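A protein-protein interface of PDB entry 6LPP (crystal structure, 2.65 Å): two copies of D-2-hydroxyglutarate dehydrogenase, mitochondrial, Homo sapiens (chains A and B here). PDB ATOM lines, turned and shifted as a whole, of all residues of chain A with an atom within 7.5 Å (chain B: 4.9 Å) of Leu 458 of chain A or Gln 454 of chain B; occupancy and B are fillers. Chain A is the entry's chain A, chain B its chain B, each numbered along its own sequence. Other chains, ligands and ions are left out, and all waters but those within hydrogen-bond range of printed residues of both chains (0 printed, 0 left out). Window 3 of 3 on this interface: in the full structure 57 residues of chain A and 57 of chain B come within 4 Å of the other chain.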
ATOM      1  N   LEU A 184      13.007   3.184  15.314  1.00  0.00           N
ATOM      2  CA  LEU A 184      12.384   3.357  14.011  1.00  0.00           C
ATOM      3  C   LEU A 184      12.202   2.013  13.301  1.00  0.00           C
ATOM      4  O   LEU A 184      12.727   0.977  13.720  1.00  0.00           O
ATOM      5  CB  LEU A 184      13.216   4.298  13.141  1.00  0.00           C
ATOM      6  CG  LEU A 184      13.532   5.677  13.726  1.00  0.00           C
ATOM      7  CD1 LEU A 184      14.394   6.488  12.767  1.00  0.00           C
ATOM      8  CD2 LEU A 184      12.250   6.420  14.059  1.00  0.00           C
ATOM      9  N   TYR A 203      15.093  20.970  15.480  1.00  0.00           N
ATOM     10  CA  TYR A 203      13.686  20.601  15.400  1.00  0.00           C
ATOM     11  C   TYR A 203      13.305  19.718  16.580  1.00  0.00           C
ATOM     12  O   TYR A 203      14.096  18.893  17.047  1.00  0.00           O
ATOM     13  CB  TYR A 203      13.376  19.860  14.097  1.00  0.00           C
ATOM     14  CG  TYR A 203      13.777  20.554  12.813  1.00  0.00           C
ATOM     15  CD1 TYR A 203      13.872  21.938  12.737  1.00  0.00           C
ATOM     16  CD2 TYR A 203      14.026  19.818  11.661  1.00  0.00           C
ATOM     17  CE1 TYR A 203      14.227  22.564  11.554  1.00  0.00           C
ATOM     18  CE2 TYR A 203      14.378  20.433  10.478  1.00  0.00           C
ATOM     19  CZ  TYR A 203      14.479  21.805  10.429  1.00  0.00           C
ATOM     20  OH  TYR A 203      14.830  22.419   9.249  1.00  0.00           O
ATOM     21  N   LEU A 208       6.878  14.611  16.719  1.00  0.00           N
ATOM     22  CA  LEU A 208       6.322  13.729  15.696  1.00  0.00           C
ATOM     23  C   LEU A 208       5.789  12.428  16.273  1.00  0.00           C
ATOM     24  O   LEU A 208       4.829  11.861  15.738  1.00  0.00           O
ATOM     25  CB  LEU A 208       7.372  13.422  14.628  1.00  0.00           C
ATOM     26  CG  LEU A 208       7.717  14.558  13.677  1.00  0.00           C
ATOM     27  CD1 LEU A 208       8.797  14.120  12.708  1.00  0.00           C
ATOM     28  CD2 LEU A 208       6.454  14.940  12.932  1.00  0.00           C
ATOM     29  N   LEU A 216       4.965   5.702  13.231  1.00  0.00           N
ATOM     30  CA  LEU A 216       6.225   6.320  12.847  1.00  0.00           C
ATOM     31  C   LEU A 216       7.418   5.763  13.610  1.00  0.00           C
ATOM     32  O   LEU A 216       8.559   6.052  13.237  1.00  0.00           O
ATOM     33  CB  LEU A 216       6.160   7.841  13.054  1.00  0.00           C
ATOM     34  CG  LEU A 216       5.084   8.607  12.283  1.00  0.00           C
ATOM     35  CD1 LEU A 216       5.168  10.098  12.578  1.00  0.00           C
ATOM     36  CD2 LEU A 216       5.207   8.348  10.789  1.00  0.00           C
ATOM     37  N   MET A 452       0.945  14.142   6.164  1.00  0.00           N
ATOM     38  CA  MET A 452       1.017  13.014   7.093  1.00  0.00           C
ATOM     39  C   MET A 452       1.487  11.749   6.382  1.00  0.00           C
ATOM     40  O   MET A 452       2.358  11.022   6.879  1.00  0.00           O
ATOM     41  CB  MET A 452      -0.342  12.783   7.755  1.00  0.00           C
ATOM     42  CG  MET A 452      -0.823  13.918   8.642  1.00  0.00           C
ATOM     43  SD  MET A 452      -2.377  13.519   9.471  1.00  0.00           S
ATOM     44  CE  MET A 452      -2.867  15.132  10.075  1.00  0.00           C
ATOM     45  N   GLN A 453       0.898  11.464   5.218  1.00  0.00           N
ATOM     46  CA  GLN A 453       1.311  10.298   4.438  1.00  0.00           C
ATOM     47  C   GLN A 453       2.762  10.405   3.975  1.00  0.00           C
ATOM     48  O   GLN A 453       3.486   9.402   3.943  1.00  0.00           O
ATOM     49  CB  GLN A 453       0.379  10.107   3.241  1.00  0.00           C
ATOM     50  CG  GLN A 453       0.692   8.868   2.413  1.00  0.00           C
ATOM     51  CD  GLN A 453       0.674   7.593   3.240  1.00  0.00           C
ATOM     52  OE1 GLN A 453      -0.245   7.362   4.025  1.00  0.00           O
ATOM     53  NE2 GLN A 453       1.697   6.762   3.070  1.00  0.00           N
ATOM     54  N   GLN A 454       3.208  11.613   3.624  1.00  0.00           N
ATOM     55  CA  GLN A 454       4.606  11.797   3.238  1.00  0.00           C
ATOM     56  C   GLN A 454       5.552  11.523   4.401  1.00  0.00           C
ATOM     57  O   GLN A 454       6.615  10.913   4.219  1.00  0.00           O
ATOM     58  CB  GLN A 454       4.829  13.216   2.713  1.00  0.00           C
ATOM     59  CG  GLN A 454       4.098  13.549   1.429  1.00  0.00           C
ATOM     60  CD  GLN A 454       4.293  14.996   1.022  1.00  0.00           C
ATOM     61  OE1 GLN A 454       3.405  15.830   1.204  1.00  0.00           O
ATOM     62  NE2 GLN A 454       5.463  15.304   0.474  1.00  0.00           N
ATOM     63  N   LEU A 455       5.178  11.952   5.606  1.00  0.00           N
ATOM     64  CA  LEU A 455       6.005  11.655   6.771  1.00  0.00           C
ATOM     65  C   LEU A 455       6.030  10.159   7.055  1.00  0.00           C
ATOM     66  O   LEU A 455       7.085   9.600   7.386  1.00  0.00           O
ATOM     67  CB  LEU A 455       5.505  12.426   7.991  1.00  0.00           C
ATOM     68  CG  LEU A 455       5.731  13.936   7.961  1.00  0.00           C
ATOM     69  CD1 LEU A 455       4.885  14.613   9.020  1.00  0.00           C
ATOM     70  CD2 LEU A 455       7.201  14.262   8.151  1.00  0.00           C
ATOM     71  N   LYS A 456       4.871   9.503   6.958  1.00  0.00           N
ATOM     72  CA  LYS A 456       4.822   8.051   7.097  1.00  0.00           C
ATOM     73  C   LYS A 456       5.753   7.366   6.101  1.00  0.00           C
ATOM     74  O   LYS A 456       6.489   6.440   6.462  1.00  0.00           O
ATOM     75  CB  LYS A 456       3.385   7.565   6.912  1.00  0.00           C
ATOM     76  CG  LYS A 456       3.216   6.055   6.857  1.00  0.00           C
ATOM     77  CD  LYS A 456       3.755   5.387   8.110  1.00  0.00           C
ATOM     78  CE  LYS A 456       3.624   3.877   8.025  1.00  0.00           C
ATOM     79  NZ  LYS A 456       3.847   3.225   9.344  1.00  0.00           N
ATOM     80  N   ALA A 457       5.737   7.814   4.844  1.00  0.00           N
ATOM     81  CA  ALA A 457       6.599   7.223   3.823  1.00  0.00           C
ATOM     82  C   ALA A 457       8.077   7.478   4.092  1.00  0.00           C
ATOM     83  O   ALA A 457       8.915   6.620   3.795  1.00  0.00           O
ATOM     84  CB  ALA A 457       6.219   7.758   2.442  1.00  0.00           C
ATOM     85  N   LEU A 458       8.414   8.641   4.652  1.00  0.00           N
ATOM     86  CA  LEU A 458       9.804   8.917   5.005  1.00  0.00           C
ATOM     87  C   LEU A 458      10.277   8.037   6.156  1.00  0.00           C
ATOM     88  O   LEU A 458      11.361   7.443   6.091  1.00  0.00           O
ATOM     89  CB  LEU A 458       9.979  10.396   5.352  1.00  0.00           C
ATOM     90  CG  LEU A 458      11.332  10.799   5.948  1.00  0.00           C
ATOM     91  CD1 LEU A 458      12.479  10.416   5.020  1.00  0.00           C
ATOM     92  CD2 LEU A 458      11.369  12.289   6.258  1.00  0.00           C
ATOM     93  N   LEU A 459       9.480   7.937   7.220  1.00  0.00           N
ATOM     94  CA  LEU A 459       9.930   7.242   8.424  1.00  0.00           C
ATOM     95  C   LEU A 459       9.773   5.728   8.331  1.00  0.00           C
ATOM     96  O   LEU A 459      10.524   4.995   8.984  1.00  0.00           O
ATOM     97  CB  LEU A 459       9.188   7.775   9.650  1.00  0.00           C
ATOM     98  CG  LEU A 459       9.624   9.170  10.101  1.00  0.00           C
ATOM     99  CD1 LEU A 459       8.648   9.758  11.107  1.00  0.00           C
ATOM    100  CD2 LEU A 459      11.027   9.115  10.684  1.00  0.00           C
ATOM    101  N   ASP A 460       8.819   5.237   7.540  1.00  0.00           N
ATOM    102  CA  ASP A 460       8.541   3.801   7.453  1.00  0.00           C
ATOM    103  C   ASP A 460       8.129   3.475   6.023  1.00  0.00           C
ATOM    104  O   ASP A 460       6.955   3.208   5.734  1.00  0.00           O
ATOM    105  CB  ASP A 460       7.464   3.402   8.464  1.00  0.00           C
ATOM    106  CG  ASP A 460       7.053   1.944   8.351  1.00  0.00           C
ATOM    107  OD1 ASP A 460       7.856   1.127   7.853  1.00  0.00           O
ATOM    108  OD2 ASP A 460       5.927   1.615   8.782  1.00  0.00           O
ATOM    109  N   PRO A 461       9.083   3.515   5.085  1.00  0.00           N
ATOM    110  CA  PRO A 461       8.738   3.280   3.670  1.00  0.00           C
ATOM    111  C   PRO A 461       8.105   1.927   3.388  1.00  0.00           C
ATOM    112  O   PRO A 461       7.273   1.829   2.477  1.00  0.00           O
ATOM    113  CB  PRO A 461      10.090   3.419   2.954  1.00  0.00           C
ATOM    114  CG  PRO A 461      11.128   3.271   4.027  1.00  0.00           C
ATOM    115  CD  PRO A 461      10.510   3.827   5.264  1.00  0.00           C
ATOM    116  N   LYS A 462       8.465   0.878   4.129  1.00  0.00           N
ATOM    117  CA  LYS A 462       7.830  -0.420   3.933  1.00  0.00           C
ATOM    118  C   LYS A 462       6.451  -0.514   4.574  1.00  0.00           C
ATOM    119  O   LYS A 462       5.710  -1.453   4.267  1.00  0.00           O
ATOM    120  CB  LYS A 462       8.721  -1.544   4.470  1.00  0.00           C
ATOM    121  CG  LYS A 462      10.061  -1.675   3.763  1.00  0.00           C
ATOM    122  CD  LYS A 462      10.746  -2.986   4.124  1.00  0.00           C
ATOM    123  CE  LYS A 462      12.098  -3.117   3.441  1.00  0.00           C
ATOM    124  NZ  LYS A 462      12.623  -4.509   3.511  1.00  0.00           N
ATOM    125  N   GLN B 450      20.455  13.917  11.604  1.00  0.00           N
ATOM    126  CA  GLN B 450      20.189  13.355  10.285  1.00  0.00           C
ATOM    127  C   GLN B 450      18.697  13.355   9.988  1.00  0.00           C
ATOM    128  O   GLN B 450      18.283  13.668   8.864  1.00  0.00           O
ATOM    129  CB  GLN B 450      20.758  11.938  10.196  1.00  0.00           C
ATOM    130  CG  GLN B 450      20.663  11.308   8.816  1.00  0.00           C
ATOM    131  CD  GLN B 450      20.943   9.816   8.836  1.00  0.00           C
ATOM    132  OE1 GLN B 450      21.494   9.289   9.803  1.00  0.00           O
ATOM    133  NE2 GLN B 450      20.559   9.126   7.767  1.00  0.00           N
ATOM    134  N   LEU B 451      17.879  12.943  10.959  1.00  0.00           N
ATOM    135  CA  LEU B 451      16.436  12.971  10.743  1.00  0.00           C
ATOM    136  C   LEU B 451      15.951  14.392  10.471  1.00  0.00           C
ATOM    137  O   LEU B 451      15.050  14.608   9.651  1.00  0.00           O
ATOM    138  CB  LEU B 451      15.706  12.374  11.946  1.00  0.00           C
ATOM    139  CG  LEU B 451      14.179  12.402  11.858  1.00  0.00           C
ATOM    140  CD1 LEU B 451      13.701  11.687  10.601  1.00  0.00           C
ATOM    141  CD2 LEU B 451      13.556  11.788  13.096  1.00  0.00           C
ATOM    142  N   MET B 452      16.555  15.379  11.143  1.00  0.00           N
ATOM    143  CA  MET B 452      16.245  16.781  10.868  1.00  0.00           C
ATOM    144  C   MET B 452      16.595  17.154   9.430  1.00  0.00           C
ATOM    145  O   MET B 452      15.828  17.851   8.749  1.00  0.00           O
ATOM    146  CB  MET B 452      17.010  17.643  11.874  1.00  0.00           C
ATOM    147  CG  MET B 452      16.493  17.464  13.301  1.00  0.00           C
ATOM    148  SD  MET B 452      17.436  18.244  14.631  1.00  0.00           S
ATOM    149  CE  MET B 452      17.938  19.786  13.895  1.00  0.00           C
ATOM    150  N   GLN B 453      17.743  16.675   8.946  1.00  0.00           N
ATOM    151  CA  GLN B 453      18.143  16.947   7.567  1.00  0.00           C
ATOM    152  C   GLN B 453      17.171  16.308   6.580  1.00  0.00           C
ATOM    153  O   GLN B 453      16.838  16.901   5.546  1.00  0.00           O
ATOM    154  CB  GLN B 453      19.577  16.476   7.330  1.00  0.00           C
ATOM    155  CG  GLN B 453      20.585  17.175   8.231  1.00  0.00           C
ATOM    156  CD  GLN B 453      21.975  16.580   8.148  1.00  0.00           C
ATOM    157  OE1 GLN B 453      22.286  15.822   7.229  1.00  0.00           O
ATOM    158  NE2 GLN B 453      22.825  16.930   9.106  1.00  0.00           N
ATOM    159  N   GLN B 454      16.704  15.096   6.891  1.00  0.00           N
ATOM    160  CA  GLN B 454      15.722  14.432   6.038  1.00  0.00           C
ATOM    161  C   GLN B 454      14.395  15.180   6.028  1.00  0.00           C
ATOM    162  O   GLN B 454      13.737  15.271   4.986  1.00  0.00           O
ATOM    163  CB  GLN B 454      15.502  12.998   6.516  1.00  0.00           C
ATOM    164  CG  GLN B 454      16.698  12.079   6.378  1.00  0.00           C
ATOM    165  CD  GLN B 454      16.479  10.750   7.076  1.00  0.00           C
ATOM    166  OE1 GLN B 454      16.948  10.539   8.194  1.00  0.00           O
ATOM    167  NE2 GLN B 454      15.755   9.850   6.421  1.00  0.00           N
ATOM    168  N   LEU B 455      13.977  15.711   7.180  1.00  0.00           N
ATOM    169  CA  LEU B 455      12.772  16.535   7.215  1.00  0.00           C
ATOM    170  C   LEU B 455      12.924  17.761   6.326  1.00  0.00           C
ATOM    171  O   LEU B 455      12.010  18.113   5.569  1.00  0.00           O
ATOM    172  CB  LEU B 455      12.441  16.944   8.649  1.00  0.00           C
ATOM    173  CG  LEU B 455      11.911  15.822   9.538  1.00  0.00           C
ATOM    174  CD1 LEU B 455      11.630  16.343  10.932  1.00  0.00           C
ATOM    175  CD2 LEU B 455      10.664  15.197   8.933  1.00  0.00           C
ATOM    176  N   LYS B 456      14.079  18.427   6.412  1.00  0.00           N
ATOM    177  CA  LYS B 456      14.344  19.584   5.561  1.00  0.00           C
ATOM    178  C   LYS B 456      14.269  19.209   4.086  1.00  0.00           C
ATOM    179  O   LYS B 456      13.650  19.916   3.282  1.00  0.00           O
ATOM    180  CB  LYS B 456      15.721  20.157   5.896  1.00  0.00           C
ATOM    181  CG  LYS B 456      16.199  21.302   5.011  1.00  0.00           C
ATOM    182  CD  LYS B 456      15.314  22.531   5.098  1.00  0.00           C
ATOM    183  CE  LYS B 456      15.815  23.612   4.149  1.00  0.00           C
ATOM    184  NZ  LYS B 456      15.090  24.901   4.316  1.00  0.00           N
ATOM    185  N   ALA B 457      14.904  18.097   3.713  1.00  0.00           N
ATOM    186  CA  ALA B 457      14.880  17.651   2.322  1.00  0.00           C
ATOM    187  C   ALA B 457      13.467  17.323   1.849  1.00  0.00           C
ATOM    188  O   ALA B 457      13.101  17.635   0.709  1.00  0.00           O
ATOM    189  CB  ALA B 457      15.796  16.440   2.148  1.00  0.00           C
ATOM    190  N   LEU B 458      12.660  16.687   2.702  1.00  0.00           N
ATOM    191  CA  LEU B 458      11.268  16.413   2.348  1.00  0.00           C
ATOM    192  C   LEU B 458      10.479  17.701   2.134  1.00  0.00           C
ATOM    193  O   LEU B 458       9.761  17.843   1.137  1.00  0.00           O
ATOM    194  CB  LEU B 458      10.613  15.545   3.428  1.00  0.00           C
ATOM    195  CG  LEU B 458       9.126  15.174   3.324  1.00  0.00           C
ATOM    196  CD1 LEU B 458       8.879  13.848   4.024  1.00  0.00           C
ATOM    197  CD2 LEU B 458       8.198  16.237   3.902  1.00  0.00           C
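SD of Met 452 of chain B lies close to N of Tyr 203 of chain A (3.7 Å).
The side-chain amide oxygen (OE1) of Gln 454 of chain B lies close to the backbone carbonyl oxygen (O) of Gln 450 of chain B (3.5 Å).
Among the printed residues, pairs that only touch across the chains: Gln 454 of chain A with Leu 458 of chain B (3.7 Å), Leu 455 of chain A with Leu 455 of chain B (3.7 Å), Leu 458 of chain A with Gln 454 of chain B (3.6 Å), Leu 458 of chain A with Leu 458 of chain B (3.7 Å) and Leu 459 of chain A with Leu 451 of chain B (3.7 Å).
Of the printed residues of chain B, Gln 454 of chain A touches Leu 458.
Of the printed residues of chain B, Leu 458 of chain A touches Gln 454 (3.6 Å) and Leu 458 (3.7 Å).
Of the printed residues of chain B, Leu 459 of chain A touches Leu 451.
Printed residues of chain A within 4 Å of Leu 451 of chain B: Leu 459.
Of chain A, only Leu 458 (3.6 Å) comes within 4 Å of Gln 454 of chain B.
Of the printed residues of chain A, Leu 455 of chain B touches Leu 455 (3.7 Å).
Lys 456 of chain B touches none of the printed residues of chain A.
Of the printed residues of chain A, Leu 458 of chain B touches Gln 454 (3.7 Å) and Leu 458 (3.7 Å).
The nearest printed residue of chain B that does not touch Leu 458 of chain A is Leu 455 of chain B (4.01 Å).
The nearest residue of chain A that does not touch Gln 454 of chain B is Leu 459 of chain A (6.4 Å).
The nearest printed residue of chain A that does not touch Leu 451 of chain B is Leu 458 of chain A (5.0 Å).
Printed residues of chain B that touch a printed residue of chain A: Leu 451, Met 452, Gln 454, Leu 455 and Leu 458.
Hydrophobic or aromatic side chains of chain B that line the printed part of chain A: Leu 451, Met 452, Leu 455 and Leu 458.
Among the printed residues, 6 pairs touch across the chains.
Gln 454 of chain A touches Leu 458 of chain B, and with the chains exchanged Leu 458 of chain A touches Gln 454 of chain B.
Leu 455 of chain B touches its own counterpart, Leu 455 of chain A.
Leu 458 of chain B touches its own counterpart, Leu 458 of chain A.
Of the 6 pairs that touch across the chains among the printed residues, 4 have their exchanged pair printed and touching as well.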
